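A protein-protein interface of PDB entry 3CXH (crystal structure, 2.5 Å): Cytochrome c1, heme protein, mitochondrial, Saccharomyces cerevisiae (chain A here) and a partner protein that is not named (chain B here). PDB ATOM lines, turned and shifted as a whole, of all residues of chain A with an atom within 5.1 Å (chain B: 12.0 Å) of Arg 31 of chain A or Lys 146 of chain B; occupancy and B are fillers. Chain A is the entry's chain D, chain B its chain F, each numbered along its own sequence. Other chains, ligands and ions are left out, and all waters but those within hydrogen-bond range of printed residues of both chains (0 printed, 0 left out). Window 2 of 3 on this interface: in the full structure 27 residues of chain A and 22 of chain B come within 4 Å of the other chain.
Of chain B, only Lys 146 (3.3 Å) comes within 4 Å of Arg 31 of chain A. Lys 146 of chain B touches just these residues of chain A: Arg 31, Thr 179, Gln 185 and Lys 188. No residue of chain B comes within 4 Å of Ala 27 of chain A. No residue of chain B comes within 4 Å of Ser 28 of chain A. No residue of chain B comes within 4 Å of Gly 32 of chain A. Gln 34 of chain A touches none of the printed residues of chain B. No residue of chain B comes within 4 Å of Val 35 of chain A. No residue of chain B comes within 4 Å of Tyr 175 of chain A. Of chain B, only Leu 145 and Lys 146 come within 4 Å of Gln 185 of chain A. No residue of chain B comes within 4 Å of Asp 189 of chain A. Of the printed residues of chain A, Leu 145 of chain B touches Gln 185 (3.3 Å) and Lys 188 (3.9 Å). Printed residues of chain B within 4 Å of Lys 188 of chain A: Phe 142, Leu 145 and Lys 146. Asp 143 of chain B touches none of the printed residues of chain A. Lys 144 of chain B touches none of the printed residues of chain A.
Of the 13 printed residues of chain B, 3 touch a printed residue of chain A. Printed residues of chain B that touch a printed residue of chain A: Phe 142, Leu 145 and Lys 146. Hydrophobic or aromatic side chains of chain B within 4 Å of the printed part of chain A: Phe 142 and Leu 145. Along chain B the printed residues that touch a printed residue of chain A span positions 142 to 146. Of the 16 printed residues of chain A, 4 touch a printed residue of chain B. Among the printed residues, 7 pairs touch across the chains.
O of Lys 146 of chain B is in salt-bridge range of NH2 of Arg 31 of chain A, at 3.99 Å. OE1 of Gln 185 of chain A sits at hydrogen-bond distance from N of Lys 146 of chain B, 3.0 Å away. NZ of Lys 188 of chain A is in salt-bridge range of O of Lys 146 of chain B (2.8 Å).
Thr 179 of chain A touches Lys 146 of chain B. Gln 185 of chain A touches Leu 145 of chain B. Lys 188 of chain A touches Phe 142 of chain B. Lys 188 of chain A touches Leu 145 of chain B (CB to CD1, 3.9 Å).
The side-chain hydroxyl of Ser 28 of chain A is in hydrogen-bond range of the side-chain amino group of Lys 188 of chain A. The guanidinium group (NH2) of Arg 31 of chain A lies close to the side-chain amide nitrogen (NE2) of Gln 185 of chain A (3.3 Å). OD2 of Asp 189 of chain A is in salt-bridge range of NH2 of Arg 31 of chain A, 3.0 Å away. OD1 of Asp 177 of chain A sits at hydrogen-bond distance from OG1 of Thr 179 of chain A, at 2.7 Å. NE2 of Gln 185 of chain A lies within hydrogen-bond range of OD2 of Asp 189 of chain A, at 3.2 Å. The side-chain amino group (NZ) of Lys 188 of chain A is in salt-bridge range of the side-chain carboxylate (OD1) of Asp 189 of chain A (3.9 Å).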
ATOM      1  N   ASP A  25     -17.013   7.411 -15.727  1.00  0.00           N
ATOM      2  CA  ASP A  25     -18.035   6.370 -15.800  1.00  0.00           C
ATOM      3  C   ASP A  25     -17.563   5.577 -17.015  1.00  0.00           C
ATOM      4  O   ASP A  25     -17.783   5.981 -18.167  1.00  0.00           O
ATOM      5  CB  ASP A  25     -19.416   6.979 -16.064  1.00  0.00           C
ATOM      6  CG  ASP A  25     -20.483   5.933 -16.392  1.00  0.00           C
ATOM      7  OD1 ASP A  25     -20.227   4.712 -16.273  1.00  0.00           O
ATOM      8  OD2 ASP A  25     -21.595   6.347 -16.784  1.00  0.00           O
ATOM      9  N   ALA A  27     -18.658   3.040 -18.399  1.00  0.00           N
ATOM     10  CA  ALA A  27     -19.721   2.520 -19.258  1.00  0.00           C
ATOM     11  C   ALA A  27     -19.993   3.580 -20.325  1.00  0.00           C
ATOM     12  O   ALA A  27     -20.202   3.267 -21.500  1.00  0.00           O
ATOM     13  CB  ALA A  27     -20.974   2.241 -18.442  1.00  0.00           C
ATOM     14  N   SER A  28     -19.962   4.839 -19.894  1.00  0.00           N
ATOM     15  CA  SER A  28     -20.170   5.984 -20.767  1.00  0.00           C
ATOM     16  C   SER A  28     -19.015   6.076 -21.781  1.00  0.00           C
ATOM     17  O   SER A  28     -19.237   6.401 -22.950  1.00  0.00           O
ATOM     18  CB  SER A  28     -20.235   7.260 -19.922  1.00  0.00           C
ATOM     19  OG  SER A  28     -20.738   8.359 -20.661  1.00  0.00           O
ATOM     20  N   ILE A  29     -17.790   5.782 -21.330  1.00  0.00           N
ATOM     21  CA  ILE A  29     -16.624   5.818 -22.209  1.00  0.00           C
ATOM     22  C   ILE A  29     -16.783   4.784 -23.309  1.00  0.00           C
ATOM     23  O   ILE A  29     -16.637   5.100 -24.487  1.00  0.00           O
ATOM     24  CB  ILE A  29     -15.307   5.549 -21.447  1.00  0.00           C
ATOM     25  CG1 ILE A  29     -15.015   6.696 -20.475  1.00  0.00           C
ATOM     26  CG2 ILE A  29     -14.147   5.406 -22.426  1.00  0.00           C
ATOM     27  CD1 ILE A  29     -13.872   6.413 -19.526  1.00  0.00           C
ATOM     28  N   ARG A  30     -17.090   3.550 -22.918  1.00  0.00           N
ATOM     29  CA  ARG A  30     -17.292   2.455 -23.867  1.00  0.00           C
ATOM     30  C   ARG A  30     -18.332   2.797 -24.941  1.00  0.00           C
ATOM     31  O   ARG A  30     -18.215   2.376 -26.088  1.00  0.00           O
ATOM     32  CB  ARG A  30     -17.725   1.190 -23.123  1.00  0.00           C
ATOM     33  CG  ARG A  30     -18.023   0.010 -24.041  1.00  0.00           C
ATOM     34  CD  ARG A  30     -18.445  -1.229 -23.262  1.00  0.00           C
ATOM     35  NE  ARG A  30     -18.621  -2.372 -24.152  1.00  0.00           N
ATOM     36  CZ  ARG A  30     -17.724  -3.339 -24.326  1.00  0.00           C
ATOM     37  NH1 ARG A  30     -17.975  -4.332 -25.168  1.00  0.00           N
ATOM     38  NH2 ARG A  30     -16.584  -3.330 -23.650  1.00  0.00           N
ATOM     39  N   ARG A  31     -19.357   3.548 -24.558  1.00  0.00           N
ATOM     40  CA  ARG A  31     -20.404   3.937 -25.488  1.00  0.00           C
ATOM     41  C   ARG A  31     -19.955   5.072 -26.397  1.00  0.00           C
ATOM     42  O   ARG A  31     -20.327   5.123 -27.581  1.00  0.00           O
ATOM     43  CB  ARG A  31     -21.653   4.359 -24.720  1.00  0.00           C
ATOM     44  CG  ARG A  31     -22.784   3.352 -24.799  1.00  0.00           C
ATOM     45  CD  ARG A  31     -23.967   3.821 -24.000  1.00  0.00           C
ATOM     46  NE  ARG A  31     -23.862   3.343 -22.634  1.00  0.00           N
ATOM     47  CZ  ARG A  31     -23.879   4.122 -21.564  1.00  0.00           C
ATOM     48  NH1 ARG A  31     -23.773   3.573 -20.361  1.00  0.00           N
ATOM     49  NH2 ARG A  31     -24.003   5.438 -21.691  1.00  0.00           N
ATOM     50  N   GLY A  32     -19.166   5.984 -25.819  1.00  0.00           N
ATOM     51  CA  GLY A  32     -18.650   7.128 -26.548  1.00  0.00           C
ATOM     52  C   GLY A  32     -17.759   6.711 -27.691  1.00  0.00           C
ATOM     53  O   GLY A  32     -17.752   7.358 -28.743  1.00  0.00           O
ATOM     54  N   TYR A  33     -17.004   5.633 -27.478  1.00  0.00           N
ATOM     55  CA  TYR A  33     -16.119   5.108 -28.503  1.00  0.00           C
ATOM     56  C   TYR A  33     -16.982   4.729 -29.702  1.00  0.00           C
ATOM     57  O   TYR A  33     -16.705   5.123 -30.843  1.00  0.00           O
ATOM     58  CB  TYR A  33     -15.354   3.862 -28.011  1.00  0.00           C
ATOM     59  CG  TYR A  33     -14.491   3.267 -29.101  1.00  0.00           C
ATOM     60  CD1 TYR A  33     -13.246   3.813 -29.399  1.00  0.00           C
ATOM     61  CD2 TYR A  33     -14.984   2.266 -29.940  1.00  0.00           C
ATOM     62  CE1 TYR A  33     -12.515   3.398 -30.516  1.00  0.00           C
ATOM     63  CE2 TYR A  33     -14.263   1.842 -31.062  1.00  0.00           C
ATOM     64  CZ  TYR A  33     -13.031   2.418 -31.346  1.00  0.00           C
ATOM     65  OH  TYR A  33     -12.336   2.043 -32.470  1.00  0.00           O
ATOM     66  N   GLN A  34     -18.035   3.964 -29.422  1.00  0.00           N
ATOM     67  CA  GLN A  34     -18.964   3.509 -30.454  1.00  0.00           C
ATOM     68  C   GLN A  34     -19.482   4.697 -31.246  1.00  0.00           C
ATOM     69  O   GLN A  34     -19.510   4.673 -32.472  1.00  0.00           O
ATOM     70  CB  GLN A  34     -20.122   2.740 -29.814  1.00  0.00           C
ATOM     71  CG  GLN A  34     -21.060   2.081 -30.803  1.00  0.00           C
ATOM     72  CD  GLN A  34     -21.976   1.047 -30.155  1.00  0.00           C
ATOM     73  OE1 GLN A  34     -21.798   0.668 -28.990  1.00  0.00           O
ATOM     74  NE2 GLN A  34     -22.954   0.576 -30.916  1.00  0.00           N
ATOM     75  N   VAL A  35     -19.838   5.760 -30.539  1.00  0.00           N
ATOM     76  CA  VAL A  35     -20.341   6.957 -31.189  1.00  0.00           C
ATOM     77  C   VAL A  35     -19.239   7.581 -32.033  1.00  0.00           C
ATOM     78  O   VAL A  35     -19.507   8.039 -33.141  1.00  0.00           O
ATOM     79  CB  VAL A  35     -20.847   7.994 -30.167  1.00  0.00           C
ATOM     80  CG1 VAL A  35     -21.507   9.168 -30.883  1.00  0.00           C
ATOM     81  CG2 VAL A  35     -21.804   7.352 -29.190  1.00  0.00           C
ATOM     82  N   TYR A 175     -26.797   1.283 -29.554  1.00  0.00           N
ATOM     83  CA  TYR A 175     -25.964   0.908 -28.419  1.00  0.00           C
ATOM     84  C   TYR A 175     -26.033  -0.574 -28.065  1.00  0.00           C
ATOM     85  O   TYR A 175     -27.110  -1.162 -28.009  1.00  0.00           O
ATOM     86  CB  TYR A 175     -26.318   1.756 -27.197  1.00  0.00           C
ATOM     87  CG  TYR A 175     -25.732   3.154 -27.203  1.00  0.00           C
ATOM     88  CD1 TYR A 175     -26.426   4.221 -26.636  1.00  0.00           C
ATOM     89  CD2 TYR A 175     -24.460   3.400 -27.717  1.00  0.00           C
ATOM     90  CE1 TYR A 175     -25.866   5.497 -26.572  1.00  0.00           C
ATOM     91  CE2 TYR A 175     -23.888   4.675 -27.656  1.00  0.00           C
ATOM     92  CZ  TYR A 175     -24.595   5.714 -27.081  1.00  0.00           C
ATOM     93  OH  TYR A 175     -24.029   6.964 -26.992  1.00  0.00           O
ATOM     94  N   ASP A 177     -25.509  -2.088 -25.189  1.00  0.00           N
ATOM     95  CA  ASP A 177     -26.238  -2.342 -23.947  1.00  0.00           C
ATOM     96  C   ASP A 177     -27.712  -1.918 -23.965  1.00  0.00           C
ATOM     97  O   ASP A 177     -28.371  -1.905 -22.923  1.00  0.00           O
ATOM     98  CB  ASP A 177     -25.497  -1.736 -22.736  1.00  0.00           C
ATOM     99  CG  ASP A 177     -25.301  -0.216 -22.831  1.00  0.00           C
ATOM    100  OD1 ASP A 177     -25.940   0.464 -23.663  1.00  0.00           O
ATOM    101  OD2 ASP A 177     -24.495   0.307 -22.033  1.00  0.00           O
ATOM    102  N   THR A 179     -29.081   1.075 -24.446  1.00  0.00           N
ATOM    103  CA  THR A 179     -29.359   2.381 -23.858  1.00  0.00           C
ATOM    104  C   THR A 179     -30.036   3.281 -24.891  1.00  0.00           C
ATOM    105  O   THR A 179     -29.634   3.299 -26.054  1.00  0.00           O
ATOM    106  CB  THR A 179     -28.047   3.042 -23.388  1.00  0.00           C
ATOM    107  OG1 THR A 179     -27.489   2.284 -22.308  1.00  0.00           O
ATOM    108  CG2 THR A 179     -28.277   4.481 -22.954  1.00  0.00           C
ATOM    109  N   GLN A 185     -27.865  11.766 -25.317  1.00  0.00           N
ATOM    110  CA  GLN A 185     -27.250  10.600 -24.688  1.00  0.00           C
ATOM    111  C   GLN A 185     -25.922  10.334 -25.392  1.00  0.00           C
ATOM    112  O   GLN A 185     -24.923  10.027 -24.744  1.00  0.00           O
ATOM    113  CB  GLN A 185     -28.140   9.359 -24.803  1.00  0.00           C
ATOM    114  CG  GLN A 185     -27.546   8.096 -24.160  1.00  0.00           C
ATOM    115  CD  GLN A 185     -27.359   8.235 -22.652  1.00  0.00           C
ATOM    116  OE1 GLN A 185     -28.252   8.713 -21.943  1.00  0.00           O
ATOM    117  NE2 GLN A 185     -26.192   7.823 -22.157  1.00  0.00           N
ATOM    118  N   LYS A 188     -23.241  12.996 -24.566  1.00  0.00           N
ATOM    119  CA  LYS A 188     -22.722  12.771 -23.224  1.00  0.00           C
ATOM    120  C   LYS A 188     -21.723  11.623 -23.247  1.00  0.00           C
ATOM    121  O   LYS A 188     -20.745  11.623 -22.510  1.00  0.00           O
ATOM    122  CB  LYS A 188     -23.877  12.466 -22.263  1.00  0.00           C
ATOM    123  CG  LYS A 188     -23.486  12.213 -20.823  1.00  0.00           C
ATOM    124  CD  LYS A 188     -23.553  10.737 -20.496  1.00  0.00           C
ATOM    125  CE  LYS A 188     -23.296  10.493 -19.028  1.00  0.00           C
ATOM    126  NZ  LYS A 188     -23.106   9.045 -18.771  1.00  0.00           N
ATOM    127  N   ASP A 189     -21.959  10.646 -24.109  1.00  0.00           N
ATOM    128  CA  ASP A 189     -21.053   9.519 -24.188  1.00  0.00           C
ATOM    129  C   ASP A 189     -19.765   9.833 -24.958  1.00  0.00           C
ATOM    130  O   ASP A 189     -18.682   9.494 -24.467  1.00  0.00           O
ATOM    131  CB  ASP A 189     -21.786   8.273 -24.694  1.00  0.00           C
ATOM    132  CG  ASP A 189     -22.861   7.787 -23.708  1.00  0.00           C
ATOM    133  OD1 ASP A 189     -22.731   8.064 -22.495  1.00  0.00           O
ATOM    134  OD2 ASP A 189     -23.839   7.141 -24.141  1.00  0.00           O
ATOM    135  N   VAL B  73     -38.472   6.651 -27.267  1.00  0.00           N
ATOM    136  CA  VAL B  73     -37.939   7.725 -26.378  1.00  0.00           C
ATOM    137  C   VAL B  73     -37.452   8.909 -27.202  1.00  0.00           C
ATOM    138  O   VAL B  73     -36.700   8.742 -28.164  1.00  0.00           O
ATOM    139  CB  VAL B  73     -36.752   7.222 -25.512  1.00  0.00           C
ATOM    140  CG1 VAL B  73     -36.359   8.277 -24.477  1.00  0.00           C
ATOM    141  CG2 VAL B  73     -37.106   5.913 -24.825  1.00  0.00           C
ATOM    142  N   THR B  74     -37.903  10.103 -26.834  1.00  0.00           N
ATOM    143  CA  THR B  74     -37.502  11.329 -27.513  1.00  0.00           C
ATOM    144  C   THR B  74     -36.363  11.979 -26.710  1.00  0.00           C
ATOM    145  O   THR B  74     -36.244  11.744 -25.500  1.00  0.00           O
ATOM    146  CB  THR B  74     -38.689  12.295 -27.628  1.00  0.00           C
ATOM    147  OG1 THR B  74     -38.236  13.571 -28.104  1.00  0.00           O
ATOM    148  CG2 THR B  74     -39.375  12.455 -26.272  1.00  0.00           C
ATOM    149  N   ASP B  75     -35.535  12.787 -27.376  1.00  0.00           N
ATOM    150  CA  ASP B  75     -34.404  13.452 -26.721  1.00  0.00           C
ATOM    151  C   ASP B  75     -34.780  14.196 -25.443  1.00  0.00           C
ATOM    152  O   ASP B  75     -35.541  15.170 -25.468  1.00  0.00           O
ATOM    153  CB  ASP B  75     -33.683  14.403 -27.684  1.00  0.00           C
ATOM    154  CG  ASP B  75     -32.442  15.042 -27.058  1.00  0.00           C
ATOM    155  OD1 ASP B  75     -31.491  14.304 -26.735  1.00  0.00           O
ATOM    156  OD2 ASP B  75     -32.417  16.279 -26.879  1.00  0.00           O
ATOM    157  N   GLN B  76     -34.180  13.762 -24.339  1.00  0.00           N
ATOM    158  CA  GLN B  76     -34.427  14.333 -23.024  1.00  0.00           C
ATOM    159  C   GLN B  76     -34.155  15.832 -22.923  1.00  0.00           C
ATOM    160  O   GLN B  76     -34.893  16.561 -22.251  1.00  0.00           O
ATOM    161  CB  GLN B  76     -33.616  13.586 -21.972  1.00  0.00           C
ATOM    162  CG  GLN B  76     -33.904  12.098 -21.904  1.00  0.00           C
ATOM    163  CD  GLN B  76     -33.016  11.267 -22.809  1.00  0.00           C
ATOM    164  OE1 GLN B  76     -32.729  10.105 -22.513  1.00  0.00           O
ATOM    165  NE2 GLN B  76     -32.574  11.854 -23.916  1.00  0.00           N
ATOM    166  N   LEU B  77     -33.099  16.296 -23.583  1.00  0.00           N
ATOM    167  CA  LEU B  77     -32.771  17.715 -23.544  1.00  0.00           C
ATOM    168  C   LEU B  77     -33.834  18.529 -24.280  1.00  0.00           C
ATOM    169  O   LEU B  77     -34.278  19.570 -23.786  1.00  0.00           O
ATOM    170  CB  LEU B  77     -31.382  17.974 -24.132  1.00  0.00           C
ATOM    171  CG  LEU B  77     -30.852  19.403 -23.984  1.00  0.00           C
ATOM    172  CD1 LEU B  77     -30.785  19.795 -22.521  1.00  0.00           C
ATOM    173  CD2 LEU B  77     -29.497  19.505 -24.628  1.00  0.00           C
ATOM    174  N   LEU B  80     -36.839  18.985 -21.962  1.00  0.00           N
ATOM    175  CA  LEU B  80     -36.574  19.978 -20.932  1.00  0.00           C
ATOM    176  C   LEU B  80     -36.620  21.410 -21.464  1.00  0.00           C
ATOM    177  O   LEU B  80     -37.188  22.298 -20.825  1.00  0.00           O
ATOM    178  CB  LEU B  80     -35.231  19.694 -20.258  1.00  0.00           C
ATOM    179  CG  LEU B  80     -35.236  18.547 -19.247  1.00  0.00           C
ATOM    180  CD1 LEU B  80     -33.831  18.205 -18.828  1.00  0.00           C
ATOM    181  CD2 LEU B  80     -36.058  18.940 -18.040  1.00  0.00           C
ATOM    182  N   ARG B 140     -30.452  19.626 -14.501  1.00  0.00           N
ATOM    183  CA  ARG B 140     -31.433  18.537 -14.520  1.00  0.00           C
ATOM    184  C   ARG B 140     -31.199  17.431 -15.537  1.00  0.00           C
ATOM    185  O   ARG B 140     -31.491  16.271 -15.263  1.00  0.00           O
ATOM    186  CB  ARG B 140     -32.830  19.106 -14.766  1.00  0.00           C
ATOM    187  CG  ARG B 140     -33.209  20.217 -13.838  1.00  0.00           C
ATOM    188  CD  ARG B 140     -34.522  20.837 -14.237  1.00  0.00           C
ATOM    189  NE  ARG B 140     -34.722  22.098 -13.532  1.00  0.00           N
ATOM    190  CZ  ARG B 140     -35.738  22.352 -12.716  1.00  0.00           C
ATOM    191  NH1 ARG B 140     -35.821  23.534 -12.115  1.00  0.00           N
ATOM    192  NH2 ARG B 140     -36.680  21.435 -12.519  1.00  0.00           N
ATOM    193  N   LEU B 141     -30.683  17.795 -16.707  1.00  0.00           N
ATOM    194  CA  LEU B 141     -30.464  16.857 -17.807  1.00  0.00           C
ATOM    195  C   LEU B 141     -29.793  15.518 -17.549  1.00  0.00           C
ATOM    196  O   LEU B 141     -30.267  14.487 -18.033  1.00  0.00           O
ATOM    197  CB  LEU B 141     -29.749  17.551 -18.966  1.00  0.00           C
ATOM    198  CG  LEU B 141     -29.429  16.638 -20.152  1.00  0.00           C
ATOM    199  CD1 LEU B 141     -30.708  16.041 -20.729  1.00  0.00           C
ATOM    200  CD2 LEU B 141     -28.669  17.415 -21.208  1.00  0.00           C
ATOM    201  N   PHE B 142     -28.681  15.524 -16.823  1.00  0.00           N
ATOM    202  CA  PHE B 142     -27.965  14.279 -16.581  1.00  0.00           C
ATOM    203  C   PHE B 142     -28.659  13.272 -15.676  1.00  0.00           C
ATOM    204  O   PHE B 142     -28.312  12.088 -15.693  1.00  0.00           O
ATOM    205  CB  PHE B 142     -26.511  14.546 -16.168  1.00  0.00           C
ATOM    206  CG  PHE B 142     -25.620  14.951 -17.325  1.00  0.00           C
ATOM    207  CD1 PHE B 142     -26.101  15.782 -18.341  1.00  0.00           C
ATOM    208  CD2 PHE B 142     -24.309  14.493 -17.408  1.00  0.00           C
ATOM    209  CE1 PHE B 142     -25.298  16.148 -19.418  1.00  0.00           C
ATOM    210  CE2 PHE B 142     -23.493  14.857 -18.488  1.00  0.00           C
ATOM    211  CZ  PHE B 142     -23.995  15.687 -19.494  1.00  0.00           C
ATOM    212  N   ASP B 143     -29.657  13.726 -14.915  1.00  0.00           N
ATOM    213  CA  ASP B 143     -30.423  12.823 -14.051  1.00  0.00           C
ATOM    214  C   ASP B 143     -31.338  11.982 -14.938  1.00  0.00           C
ATOM    215  O   ASP B 143     -31.791  10.910 -14.537  1.00  0.00           O
ATOM    216  CB  ASP B 143     -31.269  13.595 -13.037  1.00  0.00           C
ATOM    217  CG  ASP B 143     -30.503  13.945 -11.770  1.00  0.00           C
ATOM    218  OD1 ASP B 143     -30.759  15.033 -11.207  1.00  0.00           O
ATOM    219  OD2 ASP B 143     -29.661  13.134 -11.324  1.00  0.00           O
ATOM    220  N   LYS B 144     -31.590  12.482 -16.150  1.00  0.00           N
ATOM    221  CA  LYS B 144     -32.433  11.807 -17.131  1.00  0.00           C
ATOM    222  C   LYS B 144     -31.641  10.976 -18.147  1.00  0.00           C
ATOM    223  O   LYS B 144     -32.219  10.414 -19.081  1.00  0.00           O
ATOM    224  CB  LYS B 144     -33.312  12.821 -17.874  1.00  0.00           C
ATOM    225  CG  LYS B 144     -34.462  13.408 -17.055  1.00  0.00           C
ATOM    226  CD  LYS B 144     -35.561  13.941 -17.981  1.00  0.00           C
ATOM    227  CE  LYS B 144     -36.739  14.527 -17.210  1.00  0.00           C
ATOM    228  NZ  LYS B 144     -36.389  15.795 -16.499  1.00  0.00           N
ATOM    229  N   LEU B 145     -30.324  10.904 -17.976  1.00  0.00           N
ATOM    230  CA  LEU B 145     -29.484  10.133 -18.892  1.00  0.00           C
ATOM    231  C   LEU B 145     -28.841   8.940 -18.197  1.00  0.00           C
ATOM    232  O   LEU B 145     -28.757   8.895 -16.969  1.00  0.00           O
ATOM    233  CB  LEU B 145     -28.388  11.013 -19.506  1.00  0.00           C
ATOM    234  CG  LEU B 145     -28.791  12.202 -20.383  1.00  0.00           C
ATOM    235  CD1 LEU B 145     -27.540  12.921 -20.865  1.00  0.00           C
ATOM    236  CD2 LEU B 145     -29.620  11.743 -21.569  1.00  0.00           C
ATOM    237  N   LYS B 146     -28.402   7.973 -18.993  1.00  0.00           N
ATOM    238  CA  LYS B 146     -27.747   6.777 -18.477  1.00  0.00           C
ATOM    239  C   LYS B 146     -26.277   7.090 -18.161  1.00  0.00           C
ATOM    240  O   LYS B 146     -25.645   7.836 -18.950  1.00  0.00           O
ATOM    241  CB  LYS B 146     -27.858   5.639 -19.501  1.00  0.00           C
ATOM    242  CG  LYS B 146     -27.017   4.391 -19.212  1.00  0.00           C
ATOM    243  CD  LYS B 146     -27.432   3.654 -17.932  1.00  0.00           C
ATOM    244  CE  LYS B 146     -26.628   2.356 -17.736  1.00  0.00           C
ATOM    245  NZ  LYS B 146     -25.150   2.555 -17.514  1.00  0.00           N
ATOM    246  OXT LYS B 146     -25.787   6.614 -17.107  1.00  0.00           O
